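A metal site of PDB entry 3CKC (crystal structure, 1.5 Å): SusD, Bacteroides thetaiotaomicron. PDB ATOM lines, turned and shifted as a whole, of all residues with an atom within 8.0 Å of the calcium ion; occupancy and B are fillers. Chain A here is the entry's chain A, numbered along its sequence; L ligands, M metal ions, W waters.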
ATOM      1  N   PHE A 191     -16.702   5.471  10.996  1.00  0.00           N
ATOM      2  CA  PHE A 191     -18.047   6.044  11.045  1.00  0.00           C
ATOM      3  C   PHE A 191     -19.086   4.944  10.825  1.00  0.00           C
ATOM      4  O   PHE A 191     -19.076   4.257   9.808  1.00  0.00           O
ATOM      5  CB  PHE A 191     -18.199   7.135   9.988  1.00  0.00           C
ATOM      6  CG  PHE A 191     -19.413   8.002  10.190  1.00  0.00           C
ATOM      7  CD1 PHE A 191     -19.483   8.880  11.275  1.00  0.00           C
ATOM      8  CD2 PHE A 191     -20.472   7.951   9.294  1.00  0.00           C
ATOM      9  CE1 PHE A 191     -20.598   9.697  11.460  1.00  0.00           C
ATOM     10  CE2 PHE A 191     -21.596   8.767   9.475  1.00  0.00           C
ATOM     11  CZ  PHE A 191     -21.661   9.635  10.551  1.00  0.00           C
ATOM     12  N   MET A 245     -30.011  14.933   6.125  1.00  0.00           N
ATOM     13  CA  MET A 245     -29.873  14.999   4.680  1.00  0.00           C
ATOM     14  C   MET A 245     -29.031  13.845   4.137  1.00  0.00           C
ATOM     15  O   MET A 245     -28.343  13.141   4.878  1.00  0.00           O
ATOM     16  CB  MET A 245     -29.288  16.356   4.285  1.00  0.00           C
ATOM     17  CG  MET A 245     -30.267  17.495   4.546  1.00  0.00           C
ATOM     18  SD  MET A 245     -29.679  19.120   4.048  1.00  0.00           S
ATOM     19  CE  MET A 245     -30.111  19.109   2.315  1.00  0.00           C
ATOM     20  N   ALA A 246     -29.098  13.662   2.816  1.00  0.00           N
ATOM     21  CA  ALA A 246     -28.426  12.554   2.141  1.00  0.00           C
ATOM     22  C   ALA A 246     -26.928  12.405   2.287  1.00  0.00           C
ATOM     23  O   ALA A 246     -26.397  11.306   2.156  1.00  0.00           O
ATOM     24  CB  ALA A 246     -28.806  12.577   0.658  1.00  0.00           C
ATOM     25  N   ASP A 247     -26.234  13.505   2.590  1.00  0.00           N
ATOM     26  CA  ASP A 247     -24.790  13.466   2.751  1.00  0.00           C
ATOM     27  C   ASP A 247     -24.370  13.583   4.219  1.00  0.00           C
ATOM     28  O   ASP A 247     -23.270  14.064   4.513  1.00  0.00           O
ATOM     29  CB  ASP A 247     -24.134  14.565   1.914  1.00  0.00           C
ATOM     30  CG  ASP A 247     -24.560  15.960   2.339  1.00  0.00           C
ATOM     31  OD1 ASP A 247     -25.656  16.114   2.925  1.00  0.00           O
ATOM     32  OD2 ASP A 247     -23.800  16.920   2.073  1.00  0.00           O
ATOM     33  N   ASN A 248     -25.222  13.124   5.138  1.00  0.00           N
ATOM     34  CA  ASN A 248     -24.865  13.210   6.553  1.00  0.00           C
ATOM     35  C   ASN A 248     -23.766  12.243   6.978  1.00  0.00           C
ATOM     36  O   ASN A 248     -23.397  12.195   8.153  1.00  0.00           O
ATOM     37  CB  ASN A 248     -26.104  13.088   7.473  1.00  0.00           C
ATOM     38  CG  ASN A 248     -26.936  11.829   7.225  1.00  0.00           C
ATOM     39  OD1 ASN A 248     -26.626  10.987   6.396  1.00  0.00           O
ATOM     40  ND2 ASN A 248     -28.035  11.716   7.981  1.00  0.00           N
ATOM     41  N   ASP A 249     -23.215  11.490   6.024  1.00  0.00           N
ATOM     42  CA  ASP A 249     -22.129  10.561   6.319  1.00  0.00           C
ATOM     43  C   ASP A 249     -20.826  11.088   5.683  1.00  0.00           C
ATOM     44  O   ASP A 249     -19.803  10.414   5.696  1.00  0.00           O
ATOM     45  CB  ASP A 249     -22.444   9.150   5.809  1.00  0.00           C
ATOM     46  CG  ASP A 249     -22.434   9.045   4.290  1.00  0.00           C
ATOM     47  OD1 ASP A 249     -22.530  10.083   3.610  1.00  0.00           O
ATOM     48  OD2 ASP A 249     -22.348   7.906   3.777  1.00  0.00           O
ATOM     49  N   GLU A 250     -20.893  12.308   5.138  1.00  0.00           N
ATOM     50  CA  GLU A 250     -19.730  12.924   4.486  1.00  0.00           C
ATOM     51  C   GLU A 250     -19.540  14.383   4.910  1.00  0.00           C
ATOM     52  O   GLU A 250     -18.420  14.899   4.899  1.00  0.00           O
ATOM     53  CB  GLU A 250     -19.868  12.848   2.970  1.00  0.00           C
ATOM     54  CG  GLU A 250     -19.807  11.448   2.404  1.00  0.00           C
ATOM     55  CD  GLU A 250     -20.183  11.411   0.935  1.00  0.00           C
ATOM     56  OE1 GLU A 250     -19.606  12.181   0.152  1.00  0.00           O
ATOM     57  OE2 GLU A 250     -21.066  10.599   0.555  1.00  0.00           O
ATOM     58  N   ILE A 262     -26.829   5.054  11.671  1.00  0.00           N
ATOM     59  CA  ILE A 262     -27.243   3.792  11.086  1.00  0.00           C
ATOM     60  C   ILE A 262     -26.994   4.108   9.615  1.00  0.00           C
ATOM     61  O   ILE A 262     -27.720   4.894   9.011  1.00  0.00           O
ATOM     62  CB  ILE A 262     -28.736   3.497  11.319  1.00  0.00           C
ATOM     63  CG1 ILE A 262     -28.971   3.191  12.808  1.00  0.00           C
ATOM     64  CG2 ILE A 262     -29.167   2.300  10.478  1.00  0.00           C
ATOM     65  CD1 ILE A 262     -30.430   3.008  13.169  1.00  0.00           C
ATOM     66  N   ARG A 263     -25.923   3.535   9.067  1.00  0.00           N
ATOM     67  CA  ARG A 263     -25.559   3.783   7.679  1.00  0.00           C
ATOM     68  C   ARG A 263     -26.605   3.271   6.706  1.00  0.00           C
ATOM     69  O   ARG A 263     -27.109   2.150   6.847  1.00  0.00           O
ATOM     70  CB  ARG A 263     -24.207   3.115   7.354  1.00  0.00           C
ATOM     71  CG  ARG A 263     -23.047   3.488   8.285  1.00  0.00           C
ATOM     72  CD  ARG A 263     -22.783   4.980   8.297  1.00  0.00           C
ATOM     73  NE  ARG A 263     -22.407   5.510   6.989  1.00  0.00           N
ATOM     74  CZ  ARG A 263     -21.218   5.367   6.417  1.00  0.00           C
ATOM     75  NH1 ARG A 263     -20.252   4.693   7.029  1.00  0.00           N
ATOM     76  NH2 ARG A 263     -20.981   5.898   5.229  1.00  0.00           N
ATOM     77  N   GLN A 264     -26.935   4.102   5.719  1.00  0.00           N
ATOM     78  CA  GLN A 264     -27.911   3.759   4.691  1.00  0.00           C
ATOM     79  C   GLN A 264     -27.329   4.200   3.354  1.00  0.00           C
ATOM     80  O   GLN A 264     -26.614   5.203   3.287  1.00  0.00           O
ATOM     81  CB  GLN A 264     -29.236   4.476   4.939  1.00  0.00           C
ATOM     82  CG  GLN A 264     -29.798   4.317   6.360  1.00  0.00           C
ATOM     83  CD  GLN A 264     -30.615   3.045   6.569  1.00  0.00           C
ATOM     84  OE1 GLN A 264     -31.807   3.103   6.861  1.00  0.00           O
ATOM     85  NE2 GLN A 264     -29.972   1.887   6.441  1.00  0.00           N
ATOM     86  N   ASP A 265     -27.631   3.460   2.291  1.00  0.00           N
ATOM     87  CA  ASP A 265     -27.147   3.790   0.951  1.00  0.00           C
ATOM     88  C   ASP A 265     -28.247   3.377  -0.028  1.00  0.00           C
ATOM     89  O   ASP A 265     -28.625   2.204  -0.091  1.00  0.00           O
ATOM     90  CB  ASP A 265     -25.861   3.002   0.650  1.00  0.00           C
ATOM     91  CG  ASP A 265     -25.119   3.515  -0.584  1.00  0.00           C
ATOM     92  OD1 ASP A 265     -25.704   4.279  -1.375  1.00  0.00           O
ATOM     93  OD2 ASP A 265     -23.944   3.129  -0.767  1.00  0.00           O
ATOM     94  N   GLY A 266     -28.763   4.341  -0.786  1.00  0.00           N
ATOM     95  CA  GLY A 266     -29.842   4.049  -1.722  1.00  0.00           C
ATOM     96  C   GLY A 266     -29.687   2.805  -2.568  1.00  0.00           C
ATOM     97  O   GLY A 266     -30.581   1.969  -2.617  1.00  0.00           O
ATOM     98  N   THR A 269     -28.952  -0.391   0.385  1.00  0.00           N
ATOM     99  CA  THR A 269     -30.017  -0.610   1.361  1.00  0.00           C
ATOM    100  C   THR A 269     -31.349  -0.741   0.609  1.00  0.00           C
ATOM    101  O   THR A 269     -32.228  -1.509   0.992  1.00  0.00           O
ATOM    102  CB  THR A 269     -30.101   0.576   2.334  1.00  0.00           C
ATOM    103  OG1 THR A 269     -28.813   0.783   2.928  1.00  0.00           O
ATOM    104  CG2 THR A 269     -31.112   0.299   3.428  1.00  0.00           C
ATOM    105  N   SER A 275     -34.363   4.595   6.619  1.00  0.00           N
ATOM    106  CA  SER A 275     -34.609   5.904   6.027  1.00  0.00           C
ATOM    107  C   SER A 275     -35.531   5.848   4.819  1.00  0.00           C
ATOM    108  O   SER A 275     -36.080   6.868   4.392  1.00  0.00           O
ATOM    109  CB  SER A 275     -33.283   6.616   5.692  1.00  0.00           C
ATOM    110  OG  SER A 275     -32.526   5.953   4.706  1.00  0.00           O
ATOM    111  N   ASN A 391     -33.854  13.376   1.123  1.00  0.00           N
ATOM    112  CA  ASN A 391     -32.897  12.657   0.296  1.00  0.00           C
ATOM    113  C   ASN A 391     -32.244  13.634  -0.687  1.00  0.00           C
ATOM    114  O   ASN A 391     -32.266  13.434  -1.896  1.00  0.00           O
ATOM    115  CB  ASN A 391     -33.556  11.520  -0.494  1.00  0.00           C
ATOM    116  CG  ASN A 391     -32.527  10.605  -1.147  1.00  0.00           C
ATOM    117  OD1 ASN A 391     -32.732  10.094  -2.254  1.00  0.00           O
ATOM    118  ND2 ASN A 391     -31.416  10.393  -0.457  1.00  0.00           N
ATOM    119  N   ARG A 393     -28.563  16.164  -0.806  1.00  0.00           N
ATOM    120  CA  ARG A 393     -27.285  16.423  -0.150  1.00  0.00           C
ATOM    121  C   ARG A 393     -27.094  17.918   0.094  1.00  0.00           C
ATOM    122  O   ARG A 393     -27.461  18.742  -0.754  1.00  0.00           O
ATOM    123  CB  ARG A 393     -26.128  15.905  -1.002  1.00  0.00           C
ATOM    124  CG  ARG A 393     -26.145  14.400  -1.236  1.00  0.00           C
ATOM    125  CD  ARG A 393     -25.050  14.000  -2.211  1.00  0.00           C
ATOM    126  NE  ARG A 393     -23.708  14.415  -1.771  1.00  0.00           N
ATOM    127  CZ  ARG A 393     -22.835  13.610  -1.171  1.00  0.00           C
ATOM    128  NH1 ARG A 393     -23.120  12.343  -0.928  1.00  0.00           N
ATOM    129  NH2 ARG A 393     -21.637  14.083  -0.827  1.00  0.00           N
ATOM    130  N   SER A 400     -27.328   8.502  -4.793  1.00  0.00           N
ATOM    131  CA  SER A 400     -27.137   7.241  -5.508  1.00  0.00           C
ATOM    132  C   SER A 400     -28.346   6.642  -6.203  1.00  0.00           C
ATOM    133  O   SER A 400     -28.175   5.847  -7.137  1.00  0.00           O
ATOM    134  CB  SER A 400     -26.569   6.170  -4.565  1.00  0.00           C
ATOM    135  OG  SER A 400     -27.594   5.638  -3.744  1.00  0.00           O
ATOM    136  N   PRO A 405     -33.499   6.348  -0.571  1.00  0.00           N
ATOM    137  CA  PRO A 405     -32.609   7.373  -0.011  1.00  0.00           C
ATOM    138  C   PRO A 405     -31.232   6.939   0.470  1.00  0.00           C
ATOM    139  O   PRO A 405     -30.999   5.786   0.818  1.00  0.00           O
ATOM    140  CB  PRO A 405     -33.429   7.948   1.124  1.00  0.00           C
ATOM    141  CG  PRO A 405     -34.127   6.742   1.650  1.00  0.00           C
ATOM    142  CD  PRO A 405     -34.598   6.048   0.366  1.00  0.00           C
ATOM    143  N   ASP A 406     -30.316   7.915   0.495  1.00  0.00           N
ATOM    144  CA  ASP A 406     -28.945   7.710   0.958  1.00  0.00           C
ATOM    145  C   ASP A 406     -28.840   8.126   2.419  1.00  0.00           C
ATOM    146  O   ASP A 406     -27.898   7.753   3.116  1.00  0.00           O
ATOM    147  CB  ASP A 406     -27.966   8.583   0.176  1.00  0.00           C
ATOM    148  CG  ASP A 406     -27.682   8.061  -1.209  1.00  0.00           C
ATOM    149  OD1 ASP A 406     -28.152   6.953  -1.533  1.00  0.00           O
ATOM    150  OD2 ASP A 406     -26.966   8.762  -1.955  1.00  0.00           O
ATOM    151  N   THR A 407     -29.804   8.918   2.861  1.00  0.00           N
ATOM    152  CA  THR A 407     -29.806   9.451   4.220  1.00  0.00           C
ATOM    153  C   THR A 407     -29.597   8.462   5.361  1.00  0.00           C
ATOM    154  O   THR A 407     -30.367   7.530   5.533  1.00  0.00           O
ATOM    155  CB  THR A 407     -31.105  10.218   4.459  1.00  0.00           C
ATOM    156  OG1 THR A 407     -31.309  11.118   3.355  1.00  0.00           O
ATOM    157  CG2 THR A 407     -31.032  11.030   5.752  1.00  0.00           C
ATOM    158  N   ASP A 408     -28.539   8.691   6.142  1.00  0.00           N
ATOM    159  CA  ASP A 408     -28.268   7.842   7.289  1.00  0.00           C
ATOM    160  C   ASP A 408     -29.234   8.275   8.386  1.00  0.00           C
ATOM    161  O   ASP A 408     -29.777   9.381   8.341  1.00  0.00           O
ATOM    162  CB  ASP A 408     -26.864   8.069   7.853  1.00  0.00           C
ATOM    163  CG  ASP A 408     -25.768   7.451   7.016  1.00  0.00           C
ATOM    164  OD1 ASP A 408     -26.058   6.842   5.969  1.00  0.00           O
ATOM    165  OD2 ASP A 408     -24.600   7.595   7.428  1.00  0.00           O
ATOM    166  N   ILE A 409     -29.432   7.410   9.374  1.00  0.00           N
ATOM    167  CA  ILE A 409     -30.281   7.745  10.508  1.00  0.00           C
ATOM    168  C   ILE A 409     -29.328   8.060  11.672  1.00  0.00           C
ATOM    169  O   ILE A 409     -28.593   7.182  12.125  1.00  0.00           O
ATOM    170  CB  ILE A 409     -31.171   6.557  10.926  1.00  0.00           C
ATOM    171  CG1 ILE A 409     -32.146   6.232   9.785  1.00  0.00           C
ATOM    172  CG2 ILE A 409     -31.919   6.884  12.213  1.00  0.00           C
ATOM    173  CD1 ILE A 409     -33.008   5.001  10.037  1.00  0.00           C
HETATM  174  C1  LIG L   1     -25.149   0.035   4.149  1.00  0.00           C
HETATM  175  O1  LIG L   1     -24.954  -0.675   2.878  1.00  0.00           O
HETATM  176  C2  LIG L   1     -25.189   1.565   4.118  1.00  0.00           C
HETATM  177  O2  LIG L   1     -24.152   2.360   3.489  1.00  0.00           O
HETATM  178  C3  LIG L   1     -23.442   3.494   4.047  1.00  0.00           C
HETATM  179  C4  LIG L   1     -23.865   4.957   3.800  1.00  0.00           C
HETATM  180  O3  LIG L   1     -23.640   5.947   4.876  1.00  0.00           O
HETATM  181  C1  LG2 L   2     -23.294   6.393   0.380  1.00  0.00           C
HETATM  182  O1  LG2 L   2     -22.400   6.836   1.433  1.00  0.00           O
HETATM  183  C2  LG2 L   2     -24.765   6.601   0.797  1.00  0.00           C
HETATM  184  O2  LG2 L   2     -24.880   7.766   1.653  1.00  0.00           O
HETATM  185 CA    CA M   1     -25.743   7.245   3.678  1.00  0.00          CA
HETATM  186  O   HOH W   1     -25.483   9.616   4.248  1.00  0.00           O
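The side-chain amide oxygen (OE1) of Gln 264 is in hydrogen-bond range of the backbone NH (N) of Ser 275 (3.0 Å).
N of Gly 266 sits at hydrogen-bond distance from OD1 of Asp 406, 2.8 Å away.
The backbone NH (N) of Asp 406 sits close to the side-chain amide nitrogen (ND2) of Asn 391 (2.9 Å).
The side-chain hydroxyl (OG) of Ser 400 lies within hydrogen-bond range of the side-chain carboxylate (OD1) of Asp 406, at 2.6 Å.
The backbone carbonyl oxygen (O) of Asp 408 sits at hydrogen-bond distance from the side-chain amide nitrogen (ND2) of Asn 248, at 2.9 Å.
The side-chain carboxylate of Asp 408 is in salt-bridge range of the guanidinium group of Arg 263 (3.1 Å).
The side-chain carboxylate (OD2) of Asp 249 lies within salt-bridge range of the guanidinium group (NH2) of Arg 263, at 2.8 Å.
The calcium ion is bound by the backbone carbonyl oxygen (O) of Gln 264, an oxygen (O2) of LG2 L2, the backbone carbonyl oxygen (O) of Asp 406, the side-chain carboxylate (OD1) of Asp 408, water W1 and an oxygen (O3) of LIG L1.
The calcium ion has six donor atoms within binding distance.
Asp 249 touches the calcium ion.
Within 4 Å of the calcium ion: Asp 249, Gln 264, Asp 406 and Asp 408.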
